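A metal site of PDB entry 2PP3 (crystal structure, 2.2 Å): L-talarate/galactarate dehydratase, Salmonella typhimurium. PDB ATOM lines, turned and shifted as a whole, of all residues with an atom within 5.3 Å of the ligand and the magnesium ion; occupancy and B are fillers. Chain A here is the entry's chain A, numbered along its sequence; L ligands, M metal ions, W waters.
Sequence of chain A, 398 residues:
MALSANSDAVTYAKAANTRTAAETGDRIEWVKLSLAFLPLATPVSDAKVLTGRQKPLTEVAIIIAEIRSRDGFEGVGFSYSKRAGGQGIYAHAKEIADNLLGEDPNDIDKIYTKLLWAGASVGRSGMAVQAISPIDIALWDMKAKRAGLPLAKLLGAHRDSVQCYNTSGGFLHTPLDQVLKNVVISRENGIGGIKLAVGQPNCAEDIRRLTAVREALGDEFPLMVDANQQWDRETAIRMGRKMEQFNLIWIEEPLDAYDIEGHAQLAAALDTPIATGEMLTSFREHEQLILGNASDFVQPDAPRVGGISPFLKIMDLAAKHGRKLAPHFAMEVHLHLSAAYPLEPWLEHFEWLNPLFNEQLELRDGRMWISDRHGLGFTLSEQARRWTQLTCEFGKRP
The side-chain carboxylate (OE2) of Glu 348 lies close to an oxygen (O1) of the ligand (2.4 Å).
An oxygen (O4) of the ligand lies within hydrogen-bond range of a ring nitrogen (NE2) of His 328 (2.6 Å).
NZ of Lys 195 sits close to O2 of the ligand, 2.8 Å away.
OD2 of Asp 46 is in hydrogen-bond range of O5 of the ligand, at 2.9 Å.
The side-chain amide oxygen of Asn 228 sits at hydrogen-bond distance from an oxygen (O5) of the ligand (3.3 Å).
NH1 of Arg 83 lies within salt-bridge range of O7 of the ligand (3.0 Å).
O7 of the ligand is in salt-bridge range of NZ of Lys 48.
O6 of the ligand lies within hydrogen-bond range of NZ of Lys 82 (3.0 Å).
OD2 of Asp 226 lies close to NZ of Lys 195 (3.6 Å).
The side-chain carboxylate (OD1) of Asp 226 lies within hydrogen-bond range of the backbone NH (N) of Asn 228 (2.9 Å).
The side-chain amino group (NZ) of Lys 195 is in salt-bridge range of the side-chain carboxylate (OE1) of Glu 252, 2.8 Å away.
The side-chain hydroxyl (OG1) of Thr 167 sits at hydrogen-bond distance from the side-chain carboxylate (OE2) of Glu 348.
The side-chain carboxylate (OE2) of Glu 348 sits close to the side-chain hydroxyl (OH) of Tyr 165, at 3.2 Å.
The backbone NH (N) of Asn 228 is in hydrogen-bond range of the backbone carbonyl oxygen (O) of Glu 253 (3.5 Å).
The side-chain amide oxygen (OE1) of Gln 54 is in hydrogen-bond range of the guanidinium group (NH1) of Arg 83, at 3.1 Å.
O of Val 44 lies within hydrogen-bond range of N of Leu 57 (2.8 Å).
Val 44 touches the ligand (CG1 to O8, 3.8 Å).
CG2 of Thr 167 touches O1 of the ligand, at 3.7 Å.
Phe 171 touches the ligand (CZ to O6, 3.6 Å).
CZ of Phe 350 touches O1 of the ligand, 2.9 Å away.
Trp 352 touches the ligand.
Hydrophobic or aromatic side chains that line the ligand: Val 44, Phe 171, His 328, Phe 350 and Trp 352.
16 residues have an atom within 4 Å of the ligand: Val 44, Asp 46, Lys 48, Lys 82, Arg 83, Thr 167, Phe 171, Lys 195, Asp 226, Asn 228, Glu 252, Glu 278, His 328, Glu 348, Phe 350 and Trp 352.
NZ of Lys 195 touches the magnesium ion (3.9 Å).
Asn 228 touches the magnesium ion.
Of the 22 residues printed, 5 come within 4 Å of the magnesium ion.
Along chain A the residues within 4 Å of the magnesium ion span positions 195 to 278.
The nearest printed residue that does not touch the magnesium ion is His 328 (4.3 Å).
The side-chain carboxylate (OE1) of Glu 278 is bound to the magnesium ion, 2.1 Å away.
The magnesium ion is bound by water W2.
OD2 of Asp 226 is bound to the magnesium ion.
O2 of the ligand binds the magnesium ion, at 2.2 Å.
An oxygen (O3) of the ligand is bound to the magnesium ion, at 2.2 Å.
The side-chain carboxylate (OE2) of Glu 252 binds the magnesium ion.
Water W3 lies within hydrogen-bond range of O4 of the ligand (2.8 Å), OE2 of Glu 278 (2.8 Å) and NH2 of Arg 304 (3.3 Å).
Water W1 lies within hydrogen-bond range of OE1 of Glu 348 and NZ of Lys 195.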
ATOM      1  N   VAL A  44      15.746   8.219  -1.318  1.00  0.00           N
ATOM      2  CA  VAL A  44      15.989   8.862  -2.597  1.00  0.00           C
ATOM      3  C   VAL A  44      16.790  10.166  -2.496  1.00  0.00           C
ATOM      4  O   VAL A  44      16.477  11.025  -1.664  1.00  0.00           O
ATOM      5  CB  VAL A  44      14.645   9.145  -3.314  1.00  0.00           C
ATOM      6  CG1 VAL A  44      14.875   9.946  -4.596  1.00  0.00           C
ATOM      7  CG2 VAL A  44      13.957   7.820  -3.637  1.00  0.00           C
ATOM      8  N   SER A  45      17.805  10.313  -3.342  1.00  0.00           N
ATOM      9  CA  SER A  45      18.635  11.520  -3.343  1.00  0.00           C
ATOM     10  C   SER A  45      18.788  12.170  -4.716  1.00  0.00           C
ATOM     11  O   SER A  45      19.248  11.524  -5.660  1.00  0.00           O
ATOM     12  CB  SER A  45      20.053  11.227  -2.831  1.00  0.00           C
ATOM     13  OG  SER A  45      20.075  10.852  -1.463  1.00  0.00           O
ATOM     14  N   ASP A  46      18.389  13.431  -4.842  1.00  0.00           N
ATOM     15  CA  ASP A  46      18.602  14.147  -6.087  1.00  0.00           C
ATOM     16  C   ASP A  46      19.705  15.163  -5.769  1.00  0.00           C
ATOM     17  O   ASP A  46      20.286  15.118  -4.681  1.00  0.00           O
ATOM     18  CB  ASP A  46      17.336  14.839  -6.620  1.00  0.00           C
ATOM     19  CG  ASP A  46      16.735  15.843  -5.641  1.00  0.00           C
ATOM     20  OD1 ASP A  46      17.442  16.313  -4.718  1.00  0.00           O
ATOM     21  OD2 ASP A  46      15.550  16.171  -5.817  1.00  0.00           O
ATOM     22  N   LYS A  48      19.654  18.117  -4.762  1.00  0.00           N
ATOM     23  CA  LYS A  48      19.407  18.909  -3.553  1.00  0.00           C
ATOM     24  C   LYS A  48      20.080  18.232  -2.348  1.00  0.00           C
ATOM     25  O   LYS A  48      20.455  18.893  -1.385  1.00  0.00           O
ATOM     26  CB  LYS A  48      17.899  19.041  -3.284  1.00  0.00           C
ATOM     27  CG  LYS A  48      17.136  19.842  -4.325  1.00  0.00           C
ATOM     28  CD  LYS A  48      15.683  20.100  -3.906  1.00  0.00           C
ATOM     29  CE  LYS A  48      14.732  18.948  -4.250  1.00  0.00           C
ATOM     30  NZ  LYS A  48      15.091  17.660  -3.602  1.00  0.00           N
ATOM     31  N   GLN A  54      19.373  19.354   1.440  1.00  0.00           N
ATOM     32  CA  GLN A  54      18.377  18.481   2.079  1.00  0.00           C
ATOM     33  C   GLN A  54      18.923  17.096   2.367  1.00  0.00           C
ATOM     34  O   GLN A  54      19.975  16.715   1.870  1.00  0.00           O
ATOM     35  CB  GLN A  54      17.145  18.309   1.172  1.00  0.00           C
ATOM     36  CG  GLN A  54      16.427  19.567   0.770  1.00  0.00           C
ATOM     37  CD  GLN A  54      15.256  19.270  -0.160  1.00  0.00           C
ATOM     38  OE1 GLN A  54      15.388  18.482  -1.094  1.00  0.00           O
ATOM     39  NE2 GLN A  54      14.115  19.906   0.075  1.00  0.00           N
ATOM     40  N   LEU A  57      15.215  11.600   0.793  1.00  0.00           N
ATOM     41  CA  LEU A  57      13.773  11.444   0.981  1.00  0.00           C
ATOM     42  C   LEU A  57      13.456   9.998   1.362  1.00  0.00           C
ATOM     43  O   LEU A  57      13.772   9.070   0.605  1.00  0.00           O
ATOM     44  CB  LEU A  57      13.039  11.807  -0.324  1.00  0.00           C
ATOM     45  CG  LEU A  57      11.507  11.772  -0.266  1.00  0.00           C
ATOM     46  CD1 LEU A  57      11.011  12.975   0.550  1.00  0.00           C
ATOM     47  CD2 LEU A  57      10.926  11.833  -1.689  1.00  0.00           C
ATOM     48  N   LYS A  82       6.690  16.182   0.038  1.00  0.00           N
ATOM     49  CA  LYS A  82       7.952  15.439   0.076  1.00  0.00           C
ATOM     50  C   LYS A  82       8.766  16.235   1.082  1.00  0.00           C
ATOM     51  O   LYS A  82       9.168  17.358   0.803  1.00  0.00           O
ATOM     52  CB  LYS A  82       8.640  15.437  -1.294  1.00  0.00           C
ATOM     53  CG  LYS A  82       7.834  14.764  -2.393  1.00  0.00           C
ATOM     54  CD  LYS A  82       8.649  14.590  -3.666  1.00  0.00           C
ATOM     55  CE  LYS A  82       7.814  13.906  -4.745  1.00  0.00           C
ATOM     56  NZ  LYS A  82       8.565  13.718  -6.027  1.00  0.00           N
ATOM     57  N   ARG A  83       8.969  15.637   2.246  1.00  0.00           N
ATOM     58  CA  ARG A  83       9.677  16.240   3.374  1.00  0.00           C
ATOM     59  C   ARG A  83       8.653  17.054   4.165  1.00  0.00           C
ATOM     60  O   ARG A  83       7.443  16.867   3.985  1.00  0.00           O
ATOM     61  CB  ARG A  83      10.885  17.081   2.906  1.00  0.00           C
ATOM     62  CG  ARG A  83      11.961  16.195   2.256  1.00  0.00           C
ATOM     63  CD  ARG A  83      13.261  16.924   1.963  1.00  0.00           C
ATOM     64  NE  ARG A  83      14.252  16.029   1.368  1.00  0.00           N
ATOM     65  CZ  ARG A  83      14.279  15.668   0.085  1.00  0.00           C
ATOM     66  NH1 ARG A  83      13.361  16.133  -0.752  1.00  0.00           N
ATOM     67  NH2 ARG A  83      15.200  14.834  -0.365  1.00  0.00           N
ATOM     68  N   TYR A 165       7.347   9.427 -19.439  1.00  0.00           N
ATOM     69  CA  TYR A 165       8.766   9.201 -19.209  1.00  0.00           C
ATOM     70  C   TYR A 165       8.977   8.827 -17.743  1.00  0.00           C
ATOM     71  O   TYR A 165       8.199   9.253 -16.880  1.00  0.00           O
ATOM     72  CB  TYR A 165       9.590  10.464 -19.569  1.00  0.00           C
ATOM     73  CG  TYR A 165       9.471  11.590 -18.556  1.00  0.00           C
ATOM     74  CD1 TYR A 165      10.253  11.610 -17.406  1.00  0.00           C
ATOM     75  CD2 TYR A 165       8.538  12.609 -18.735  1.00  0.00           C
ATOM     76  CE1 TYR A 165      10.099  12.610 -16.452  1.00  0.00           C
ATOM     77  CE2 TYR A 165       8.376  13.615 -17.778  1.00  0.00           C
ATOM     78  CZ  TYR A 165       9.168  13.610 -16.647  1.00  0.00           C
ATOM     79  OH  TYR A 165       9.023  14.612 -15.707  1.00  0.00           O
ATOM     80  N   THR A 167      11.138   8.763 -14.110  1.00  0.00           N
ATOM     81  CA  THR A 167      12.102   9.532 -13.330  1.00  0.00           C
ATOM     82  C   THR A 167      12.676   8.749 -12.146  1.00  0.00           C
ATOM     83  O   THR A 167      13.832   8.940 -11.770  1.00  0.00           O
ATOM     84  CB  THR A 167      11.444  10.815 -12.763  1.00  0.00           C
ATOM     85  OG1 THR A 167      10.973  11.620 -13.854  1.00  0.00           O
ATOM     86  CG2 THR A 167      12.436  11.607 -11.947  1.00  0.00           C
ATOM     87  N   PHE A 171      17.723   8.639 -10.336  1.00  0.00           N
ATOM     88  CA  PHE A 171      18.169   9.503  -9.249  1.00  0.00           C
ATOM     89  C   PHE A 171      19.662   9.377  -8.925  1.00  0.00           C
ATOM     90  O   PHE A 171      20.300   8.374  -9.234  1.00  0.00           O
ATOM     91  CB  PHE A 171      17.314   9.251  -8.004  1.00  0.00           C
ATOM     92  CG  PHE A 171      16.000   9.976  -8.025  1.00  0.00           C
ATOM     93  CD1 PHE A 171      15.950  11.353  -7.771  1.00  0.00           C
ATOM     94  CD2 PHE A 171      14.829   9.306  -8.316  1.00  0.00           C
ATOM     95  CE1 PHE A 171      14.736  12.039  -7.815  1.00  0.00           C
ATOM     96  CE2 PHE A 171      13.604   9.986  -8.368  1.00  0.00           C
ATOM     97  CZ  PHE A 171      13.562  11.356  -8.118  1.00  0.00           C
ATOM     98  N   LYS A 195      14.339  10.328 -17.710  1.00  0.00           N
ATOM     99  CA  LYS A 195      14.847  11.581 -17.175  1.00  0.00           C
ATOM    100  C   LYS A 195      15.945  11.234 -16.164  1.00  0.00           C
ATOM    101  O   LYS A 195      15.763  10.346 -15.327  1.00  0.00           O
ATOM    102  CB  LYS A 195      13.742  12.414 -16.512  1.00  0.00           C
ATOM    103  CG  LYS A 195      14.211  13.824 -16.111  1.00  0.00           C
ATOM    104  CD  LYS A 195      13.067  14.788 -15.781  1.00  0.00           C
ATOM    105  CE  LYS A 195      12.539  14.634 -14.357  1.00  0.00           C
ATOM    106  NZ  LYS A 195      11.325  15.469 -14.117  1.00  0.00           N
ATOM    107  N   ASP A 226      17.338  16.780 -15.133  1.00  0.00           N
ATOM    108  CA  ASP A 226      16.771  17.617 -14.095  1.00  0.00           C
ATOM    109  C   ASP A 226      17.853  18.007 -13.083  1.00  0.00           C
ATOM    110  O   ASP A 226      18.377  17.136 -12.382  1.00  0.00           O
ATOM    111  CB  ASP A 226      15.659  16.845 -13.383  1.00  0.00           C
ATOM    112  CG  ASP A 226      14.835  17.712 -12.456  1.00  0.00           C
ATOM    113  OD1 ASP A 226      15.274  18.833 -12.088  1.00  0.00           O
ATOM    114  OD2 ASP A 226      13.744  17.259 -12.083  1.00  0.00           O
ATOM    115  N   ASN A 228      17.388  20.088 -10.536  1.00  0.00           N
ATOM    116  CA  ASN A 228      16.750  20.467  -9.280  1.00  0.00           C
ATOM    117  C   ASN A 228      17.268  21.750  -8.614  1.00  0.00           C
ATOM    118  O   ASN A 228      17.535  21.761  -7.403  1.00  0.00           O
ATOM    119  CB  ASN A 228      16.800  19.300  -8.285  1.00  0.00           C
ATOM    120  CG  ASN A 228      15.792  18.214  -8.607  1.00  0.00           C
ATOM    121  OD1 ASN A 228      14.582  18.426  -8.454  1.00  0.00           O
ATOM    122  ND2 ASN A 228      16.271  17.078  -9.080  1.00  0.00           N
ATOM    123  N   GLU A 252      15.670  20.506 -17.039  1.00  0.00           N
ATOM    124  CA  GLU A 252      14.737  20.925 -16.007  1.00  0.00           C
ATOM    125  C   GLU A 252      15.348  21.580 -14.768  1.00  0.00           C
ATOM    126  O   GLU A 252      16.372  21.133 -14.264  1.00  0.00           O
ATOM    127  CB  GLU A 252      13.928  19.687 -15.584  1.00  0.00           C
ATOM    128  CG  GLU A 252      12.844  19.927 -14.564  1.00  0.00           C
ATOM    129  CD  GLU A 252      11.960  18.689 -14.416  1.00  0.00           C
ATOM    130  OE1 GLU A 252      11.830  17.934 -15.393  1.00  0.00           O
ATOM    131  OE2 GLU A 252      11.396  18.488 -13.333  1.00  0.00           O
ATOM    132  N   GLU A 253      14.671  22.610 -14.276  1.00  0.00           N
ATOM    133  CA  GLU A 253      15.134  23.354 -13.107  1.00  0.00           C
ATOM    134  C   GLU A 253      16.637  23.571 -13.048  1.00  0.00           C
ATOM    135  O   GLU A 253      17.303  23.189 -12.078  1.00  0.00           O
ATOM    136  CB  GLU A 253      14.652  22.665 -11.827  1.00  0.00           C
ATOM    137  CG  GLU A 253      13.149  22.723 -11.636  1.00  0.00           C
ATOM    138  CD  GLU A 253      12.762  22.829 -10.173  1.00  0.00           C
ATOM    139  OE1 GLU A 253      12.846  21.811  -9.440  1.00  0.00           O
ATOM    140  OE2 GLU A 253      12.368  23.947  -9.759  1.00  0.00           O
ATOM    141  N   GLU A 278       7.683  22.956 -11.056  1.00  0.00           N
ATOM    142  CA  GLU A 278       7.152  22.026 -10.065  1.00  0.00           C
ATOM    143  C   GLU A 278       7.100  22.585  -8.633  1.00  0.00           C
ATOM    144  O   GLU A 278       6.243  22.193  -7.855  1.00  0.00           O
ATOM    145  CB  GLU A 278       7.976  20.737 -10.047  1.00  0.00           C
ATOM    146  CG  GLU A 278       9.272  20.843  -9.261  1.00  0.00           C
ATOM    147  CD  GLU A 278      10.134  19.640  -9.462  1.00  0.00           C
ATOM    148  OE1 GLU A 278      10.328  19.262 -10.629  1.00  0.00           O
ATOM    149  OE2 GLU A 278      10.618  19.059  -8.472  1.00  0.00           O
ATOM    150  N   ARG A 304       0.210  20.868  -5.671  1.00  0.00           N
ATOM    151  CA  ARG A 304       0.972  22.011  -5.188  1.00  0.00           C
ATOM    152  C   ARG A 304       0.426  23.385  -5.456  1.00  0.00           C
ATOM    153  O   ARG A 304       0.652  24.292  -4.656  1.00  0.00           O
ATOM    154  CB  ARG A 304       2.412  21.936  -5.683  1.00  0.00           C
ATOM    155  CG  ARG A 304       3.255  21.030  -4.830  1.00  0.00           C
ATOM    156  CD  ARG A 304       4.681  21.041  -5.285  1.00  0.00           C
ATOM    157  NE  ARG A 304       5.506  20.192  -4.427  1.00  0.00           N
ATOM    158  CZ  ARG A 304       6.654  19.654  -4.823  1.00  0.00           C
ATOM    159  NH1 ARG A 304       7.096  19.891  -6.059  1.00  0.00           N
ATOM    160  NH2 ARG A 304       7.357  18.893  -3.991  1.00  0.00           N
ATOM    161  N   HIS A 328       4.219  17.768 -13.059  1.00  0.00           N
ATOM    162  CA  HIS A 328       5.130  17.097 -12.143  1.00  0.00           C
ATOM    163  C   HIS A 328       4.459  16.121 -11.191  1.00  0.00           C
ATOM    164  O   HIS A 328       3.513  16.486 -10.500  1.00  0.00           O
ATOM    165  CB  HIS A 328       5.887  18.149 -11.314  1.00  0.00           C
ATOM    166  CG  HIS A 328       6.607  17.588 -10.121  1.00  0.00           C
ATOM    167  ND1 HIS A 328       6.082  17.631  -8.852  1.00  0.00           N
ATOM    168  CD2 HIS A 328       7.825  17.006 -10.008  1.00  0.00           C
ATOM    169  CE1 HIS A 328       6.948  17.092  -8.007  1.00  0.00           C
ATOM    170  NE2 HIS A 328       8.014  16.704  -8.684  1.00  0.00           N
ATOM    171  N   GLU A 348       4.849  12.414 -16.219  1.00  0.00           N
ATOM    172  CA  GLU A 348       5.957  11.881 -15.436  1.00  0.00           C
ATOM    173  C   GLU A 348       5.572  10.639 -14.638  1.00  0.00           C
ATOM    174  O   GLU A 348       4.543  10.619 -13.963  1.00  0.00           O
ATOM    175  CB  GLU A 348       6.494  12.960 -14.483  1.00  0.00           C
ATOM    176  CG  GLU A 348       7.621  12.487 -13.578  1.00  0.00           C
ATOM    177  CD  GLU A 348       8.320  13.639 -12.841  1.00  0.00           C
ATOM    178  OE1 GLU A 348       7.628  14.568 -12.391  1.00  0.00           O
ATOM    179  OE2 GLU A 348       9.553  13.597 -12.705  1.00  0.00           O
ATOM    180  N   PHE A 350       6.330   7.607 -11.766  1.00  0.00           N
ATOM    181  CA  PHE A 350       6.953   7.139 -10.531  1.00  0.00           C
ATOM    182  C   PHE A 350       6.006   5.988 -10.214  1.00  0.00           C
ATOM    183  O   PHE A 350       4.830   6.063 -10.552  1.00  0.00           O
ATOM    184  CB  PHE A 350       6.834   8.144  -9.384  1.00  0.00           C
ATOM    185  CG  PHE A 350       7.807   9.296  -9.439  1.00  0.00           C
ATOM    186  CD1 PHE A 350       7.540  10.426 -10.213  1.00  0.00           C
ATOM    187  CD2 PHE A 350       8.958   9.273  -8.660  1.00  0.00           C
ATOM    188  CE1 PHE A 350       8.412  11.516 -10.206  1.00  0.00           C
ATOM    189  CE2 PHE A 350       9.834  10.348  -8.645  1.00  0.00           C
ATOM    190  CZ  PHE A 350       9.554  11.477  -9.414  1.00  0.00           C
ATOM    191  N   TRP A 352       5.834   5.055  -7.106  1.00  0.00           N
ATOM    192  CA  TRP A 352       5.649   5.341  -5.675  1.00  0.00           C
ATOM    193  C   TRP A 352       4.216   5.286  -5.127  1.00  0.00           C
ATOM    194  O   TRP A 352       3.992   4.734  -4.058  1.00  0.00           O
ATOM    195  CB  TRP A 352       6.226   6.712  -5.333  1.00  0.00           C
ATOM    196  CG  TRP A 352       7.696   6.841  -5.536  1.00  0.00           C
ATOM    197  CD1 TRP A 352       8.556   5.862  -5.974  1.00  0.00           C
ATOM    198  CD2 TRP A 352       8.490   8.002  -5.302  1.00  0.00           C
ATOM    199  NE1 TRP A 352       9.833   6.360  -6.033  1.00  0.00           N
ATOM    200  CE2 TRP A 352       9.827   7.662  -5.623  1.00  0.00           C
ATOM    201  CE3 TRP A 352       8.211   9.295  -4.852  1.00  0.00           C
ATOM    202  CZ2 TRP A 352      10.888   8.581  -5.510  1.00  0.00           C
ATOM    203  CZ3 TRP A 352       9.256  10.214  -4.743  1.00  0.00           C
ATOM    204  CH2 TRP A 352      10.576   9.847  -5.072  1.00  0.00           C
HETATM  205  O1  LIG L   1      10.227  14.139 -10.433  1.00  0.00           O
HETATM  206  C1  LIG L   1      10.901  15.178 -10.475  1.00  0.00           C
HETATM  207  O2  LIG L   1      10.875  15.986 -11.415  1.00  0.00           O
HETATM  208  C2  LIG L   1      11.879  15.489  -9.293  1.00  0.00           C
HETATM  209  O3  LIG L   1      12.217  16.880  -9.234  1.00  0.00           O
HETATM  210  C3  LIG L   1      11.314  15.087  -7.936  1.00  0.00           C
HETATM  211  O4  LIG L   1      10.285  16.008  -7.593  1.00  0.00           O
HETATM  212  C4  LIG L   1      12.366  15.098  -6.797  1.00  0.00           C
HETATM  213  O5  LIG L   1      12.775  16.456  -6.521  1.00  0.00           O
HETATM  214  C5  LIG L   1      11.884  14.468  -5.486  1.00  0.00           C
HETATM  215  O6  LIG L   1      11.513  13.109  -5.744  1.00  0.00           O
HETATM  216  C6  LIG L   1      12.983  14.505  -4.416  1.00  0.00           C
HETATM  217  O7  LIG L   1      12.993  15.514  -3.645  1.00  0.00           O
HETATM  218  O8  LIG L   1      13.805  13.557  -4.377  1.00  0.00           O
HETATM  219 MG    MG M   1      11.869  17.937 -11.182  1.00  0.00          MG
HETATM  220  O   HOH W   1       8.629  17.411 -13.349  1.00  0.00           O
HETATM  221  O   HOH W   2      13.021  19.747 -10.762  1.00  0.00           O
HETATM  222  O   HOH W   3       9.967  18.141  -5.857  1.00  0.00           O
HETATM  223  O   HOH W   4      14.900  15.263 -10.110  1.00  0.00           O
HETATM  224  O   HOH W   5      11.337  17.502  -3.444  1.00  0.00           O
